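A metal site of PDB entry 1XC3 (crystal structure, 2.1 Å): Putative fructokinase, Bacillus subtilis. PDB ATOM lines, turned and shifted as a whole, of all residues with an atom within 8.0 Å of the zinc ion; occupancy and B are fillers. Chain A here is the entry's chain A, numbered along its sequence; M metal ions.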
ATOM      1  N   ILE A 135      24.924  10.930   5.472  1.00  0.00           N
ATOM      2  CA  ILE A 135      26.234  11.580   5.456  1.00  0.00           C
ATOM      3  C   ILE A 135      27.246  10.741   6.246  1.00  0.00           C
ATOM      4  O   ILE A 135      26.982  10.358   7.383  1.00  0.00           O
ATOM      5  CB  ILE A 135      26.190  13.043   6.013  1.00  0.00           C
ATOM      6  CG1 ILE A 135      25.179  13.880   5.209  1.00  0.00           C
ATOM      7  CG2 ILE A 135      27.611  13.675   5.988  1.00  0.00           C
ATOM      8  CD1 ILE A 135      25.100  15.365   5.577  1.00  0.00           C
ATOM      9  N   GLU A 153      31.812   8.445  12.637  1.00  0.00           N
ATOM     10  CA  GLU A 153      30.436   8.665  12.156  1.00  0.00           C
ATOM     11  C   GLU A 153      30.214  10.162  12.105  1.00  0.00           C
ATOM     12  O   GLU A 153      29.376  10.729  12.841  1.00  0.00           O
ATOM     13  CB  GLU A 153      29.408   7.966  13.066  1.00  0.00           C
ATOM     14  CG  GLU A 153      29.255   6.483  12.752  1.00  0.00           C
ATOM     15  CD  GLU A 153      28.646   6.245  11.369  1.00  0.00           C
ATOM     16  OE1 GLU A 153      27.706   6.969  10.986  1.00  0.00           O
ATOM     17  OE2 GLU A 153      29.121   5.357  10.649  1.00  0.00           O
ATOM     18  N   GLY A 155      28.895  12.201  10.131  1.00  0.00           N
ATOM     19  CA  GLY A 155      27.633  12.751   9.664  1.00  0.00           C
ATOM     20  C   GLY A 155      26.635  13.047  10.769  1.00  0.00           C
ATOM     21  O   GLY A 155      25.641  13.757  10.558  1.00  0.00           O
ATOM     22  N   HIS A 156      26.890  12.526  11.969  1.00  0.00           N
ATOM     23  CA  HIS A 156      25.943  12.662  13.067  1.00  0.00           C
ATOM     24  C   HIS A 156      26.299  13.705  14.133  1.00  0.00           C
ATOM     25  O   HIS A 156      25.706  13.753  15.213  1.00  0.00           O
ATOM     26  CB  HIS A 156      25.621  11.292  13.665  1.00  0.00           C
ATOM     27  CG  HIS A 156      24.822  10.424  12.737  1.00  0.00           C
ATOM     28  ND1 HIS A 156      23.446  10.406  12.712  1.00  0.00           N
ATOM     29  CD2 HIS A 156      25.222   9.571  11.765  1.00  0.00           C
ATOM     30  CE1 HIS A 156      23.033   9.562  11.774  1.00  0.00           C
ATOM     31  NE2 HIS A 156      24.099   9.047  11.190  1.00  0.00           N
ATOM     32  N   ILE A 157      27.249  14.575  13.805  1.00  0.00           N
ATOM     33  CA  ILE A 157      27.627  15.676  14.694  1.00  0.00           C
ATOM     34  C   ILE A 157      26.547  16.752  14.690  1.00  0.00           C
ATOM     35  O   ILE A 157      25.886  16.992  13.668  1.00  0.00           O
ATOM     36  CB  ILE A 157      28.981  16.331  14.326  1.00  0.00           C
ATOM     37  CG1 ILE A 157      28.942  16.935  12.916  1.00  0.00           C
ATOM     38  CG2 ILE A 157      30.147  15.326  14.496  1.00  0.00           C
ATOM     39  CD1 ILE A 157      30.047  17.952  12.650  1.00  0.00           C
ATOM     40  N   TYR A 158      26.373  17.395  15.825  1.00  0.00           N
ATOM     41  CA  TYR A 158      25.509  18.551  15.866  1.00  0.00           C
ATOM     42  C   TYR A 158      26.234  19.749  15.220  1.00  0.00           C
ATOM     43  O   TYR A 158      27.453  19.926  15.360  1.00  0.00           O
ATOM     44  CB  TYR A 158      24.979  18.810  17.284  1.00  0.00           C
ATOM     45  CG  TYR A 158      23.855  17.849  17.704  1.00  0.00           C
ATOM     46  CD1 TYR A 158      24.056  16.874  18.703  1.00  0.00           C
ATOM     47  CD2 TYR A 158      22.586  17.911  17.098  1.00  0.00           C
ATOM     48  CE1 TYR A 158      23.023  15.980  19.081  1.00  0.00           C
ATOM     49  CE2 TYR A 158      21.546  17.033  17.472  1.00  0.00           C
ATOM     50  CZ  TYR A 158      21.772  16.081  18.468  1.00  0.00           C
ATOM     51  OH  TYR A 158      20.747  15.220  18.832  1.00  0.00           O
ATOM     52  N   LYS A 170      15.812  15.039   9.809  1.00  0.00           N
ATOM     53  CA  LYS A 170      15.484  13.700   9.313  1.00  0.00           C
ATOM     54  C   LYS A 170      16.013  12.538  10.174  1.00  0.00           C
ATOM     55  O   LYS A 170      15.482  11.430  10.122  1.00  0.00           O
ATOM     56  CB  LYS A 170      15.958  13.548   7.854  1.00  0.00           C
ATOM     57  CG  LYS A 170      15.538  12.270   7.107  1.00  0.00           C
ATOM     58  CD  LYS A 170      14.013  12.121   6.995  1.00  0.00           C
ATOM     59  CE  LYS A 170      13.613  10.980   6.061  1.00  0.00           C
ATOM     60  NZ  LYS A 170      12.164  10.569   6.248  1.00  0.00           N
ATOM     61  N   CYS A 171      17.052  12.786  10.988  1.00  0.00           N
ATOM     62  CA  CYS A 171      17.760  11.680  11.649  1.00  0.00           C
ATOM     63  C   CYS A 171      16.973  10.974  12.761  1.00  0.00           C
ATOM     64  O   CYS A 171      16.608  11.603  13.753  1.00  0.00           O
ATOM     65  CB  CYS A 171      19.126  12.123  12.195  1.00  0.00           C
ATOM     66  SG  CYS A 171      20.026  10.760  12.968  1.00  0.00           S
ATOM     67  N   PRO A 172      16.752   9.663  12.615  1.00  0.00           N
ATOM     68  CA  PRO A 172      15.960   8.902  13.593  1.00  0.00           C
ATOM     69  C   PRO A 172      16.617   8.814  14.981  1.00  0.00           C
ATOM     70  O   PRO A 172      15.927   8.571  15.969  1.00  0.00           O
ATOM     71  CB  PRO A 172      15.835   7.523  12.962  1.00  0.00           C
ATOM     72  CG  PRO A 172      16.944   7.435  11.961  1.00  0.00           C
ATOM     73  CD  PRO A 172      17.231   8.818  11.510  1.00  0.00           C
ATOM     74  N   TYR A 173      17.935   9.029  15.049  1.00  0.00           N
ATOM     75  CA  TYR A 173      18.658   9.042  16.313  1.00  0.00           C
ATOM     76  C   TYR A 173      18.729  10.424  16.968  1.00  0.00           C
ATOM     77  O   TYR A 173      18.535  10.541  18.181  1.00  0.00           O
ATOM     78  CB  TYR A 173      20.071   8.496  16.125  1.00  0.00           C
ATOM     79  CG  TYR A 173      20.173   6.996  16.059  1.00  0.00           C
ATOM     80  CD1 TYR A 173      20.126   6.324  14.825  1.00  0.00           C
ATOM     81  CD2 TYR A 173      20.311   6.229  17.228  1.00  0.00           C
ATOM     82  CE1 TYR A 173      20.247   4.925  14.769  1.00  0.00           C
ATOM     83  CE2 TYR A 173      20.412   4.834  17.169  1.00  0.00           C
ATOM     84  CZ  TYR A 173      20.383   4.195  15.937  1.00  0.00           C
ATOM     85  OH  TYR A 173      20.494   2.806  15.885  1.00  0.00           O
ATOM     86  N   HIS A 174      19.038  11.460  16.185  1.00  0.00           N
ATOM     87  CA  HIS A 174      19.374  12.774  16.751  1.00  0.00           C
ATOM     88  C   HIS A 174      18.408  13.887  16.372  1.00  0.00           C
ATOM     89  O   HIS A 174      18.395  14.938  17.009  1.00  0.00           O
ATOM     90  CB  HIS A 174      20.797  13.187  16.352  1.00  0.00           C
ATOM     91  CG  HIS A 174      21.800  12.097  16.548  1.00  0.00           C
ATOM     92  ND1 HIS A 174      22.340  11.382  15.493  1.00  0.00           N
ATOM     93  CD2 HIS A 174      22.304  11.545  17.680  1.00  0.00           C
ATOM     94  CE1 HIS A 174      23.144  10.448  15.974  1.00  0.00           C
ATOM     95  NE2 HIS A 174      23.147  10.534  17.289  1.00  0.00           N
ATOM     96  N   GLY A 175      17.625  13.648  15.324  1.00  0.00           N
ATOM     97  CA  GLY A 175      16.782  14.709  14.770  1.00  0.00           C
ATOM     98  C   GLY A 175      17.604  15.637  13.898  1.00  0.00           C
ATOM     99  O   GLY A 175      17.756  15.403  12.684  1.00  0.00           O
ATOM    100  N   ASP A 176      18.141  16.693  14.505  1.00  0.00           N
ATOM    101  CA  ASP A 176      18.839  17.745  13.757  1.00  0.00           C
ATOM    102  C   ASP A 176      20.376  17.742  13.858  1.00  0.00           C
ATOM    103  O   ASP A 176      21.007  18.795  14.009  1.00  0.00           O
ATOM    104  CB  ASP A 176      18.282  19.133  14.099  1.00  0.00           C
ATOM    105  CG  ASP A 176      18.387  19.468  15.567  1.00  0.00           C
ATOM    106  OD1 ASP A 176      18.866  18.637  16.363  1.00  0.00           O
ATOM    107  OD2 ASP A 176      18.005  20.606  15.924  1.00  0.00           O
ATOM    108  N   CYS A 177      20.986  16.556  13.746  1.00  0.00           N
ATOM    109  CA  CYS A 177      22.417  16.460  13.466  1.00  0.00           C
ATOM    110  C   CYS A 177      22.688  16.902  12.028  1.00  0.00           C
ATOM    111  O   CYS A 177      21.760  17.261  11.286  1.00  0.00           O
ATOM    112  CB  CYS A 177      22.907  15.027  13.700  1.00  0.00           C
ATOM    113  SG  CYS A 177      22.056  13.763  12.720  1.00  0.00           S
ATOM    114  N   PHE A 178      23.957  16.901  11.636  1.00  0.00           N
ATOM    115  CA  PHE A 178      24.387  17.274  10.290  1.00  0.00           C
ATOM    116  C   PHE A 178      23.600  16.488   9.224  1.00  0.00           C
ATOM    117  O   PHE A 178      22.995  17.074   8.309  1.00  0.00           O
ATOM    118  CB  PHE A 178      25.917  17.097  10.166  1.00  0.00           C
ATOM    119  CG  PHE A 178      26.492  17.413   8.807  1.00  0.00           C
ATOM    120  CD1 PHE A 178      25.899  18.364   7.962  1.00  0.00           C
ATOM    121  CD2 PHE A 178      27.673  16.803   8.396  1.00  0.00           C
ATOM    122  CE1 PHE A 178      26.453  18.648   6.724  1.00  0.00           C
ATOM    123  CE2 PHE A 178      28.238  17.094   7.165  1.00  0.00           C
ATOM    124  CZ  PHE A 178      27.619  18.021   6.323  1.00  0.00           C
ATOM    125  N   GLU A 179      23.570  15.163   9.350  1.00  0.00           N
ATOM    126  CA  GLU A 179      22.794  14.325   8.447  1.00  0.00           C
ATOM    127  C   GLU A 179      21.304  14.674   8.438  1.00  0.00           C
ATOM    128  O   GLU A 179      20.697  14.745   7.368  1.00  0.00           O
ATOM    129  CB  GLU A 179      22.943  12.846   8.786  1.00  0.00           C
ATOM    130  CG  GLU A 179      22.273  11.946   7.760  1.00  0.00           C
ATOM    131  CD  GLU A 179      22.486  10.504   8.053  1.00  0.00           C
ATOM    132  OE1 GLU A 179      23.548   9.985   7.672  1.00  0.00           O
ATOM    133  OE2 GLU A 179      21.592   9.891   8.673  1.00  0.00           O
ATOM    134  N   GLY A 180      20.741  14.881   9.618  1.00  0.00           N
ATOM    135  CA  GLY A 180      19.340  15.263   9.775  1.00  0.00           C
ATOM    136  C   GLY A 180      18.973  16.558   9.066  1.00  0.00           C
ATOM    137  O   GLY A 180      17.870  16.691   8.560  1.00  0.00           O
ATOM    138  N   LEU A 181      19.907  17.514   9.023  1.00  0.00           N
ATOM    139  CA  LEU A 181      19.672  18.804   8.405  1.00  0.00           C
ATOM    140  C   LEU A 181      20.084  18.908   6.939  1.00  0.00           C
ATOM    141  O   LEU A 181      19.559  19.756   6.215  1.00  0.00           O
ATOM    142  CB  LEU A 181      20.390  19.907   9.197  1.00  0.00           C
ATOM    143  CG  LEU A 181      19.823  20.220  10.580  1.00  0.00           C
ATOM    144  CD1 LEU A 181      20.797  21.143  11.343  1.00  0.00           C
ATOM    145  CD2 LEU A 181      18.437  20.872  10.465  1.00  0.00           C
HETATM  146 ZN    ZN M   1      22.113  11.736  13.519  1.00  0.00          ZN
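The side-chain sulfur of Cys 177 lies close to the backbone NH of Gly 180.
The backbone carbonyl oxygen of His 174 lies within hydrogen-bond range of the side-chain hydroxyl of Tyr 158.
The side-chain sulfur of Cys 171 sits close to the backbone NH of Tyr 173.
The nearest printed residue that does not touch the zinc ion is Tyr 173 (4.6 Å).
The zinc ion is bound by a ring nitrogen (ND1) of His 174, a ring nitrogen (ND1) of His 156, the side-chain sulfur (SG) of Cys 177 and the side-chain sulfur (SG) of Cys 171.
The zinc ion has four donor atoms within binding distance.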
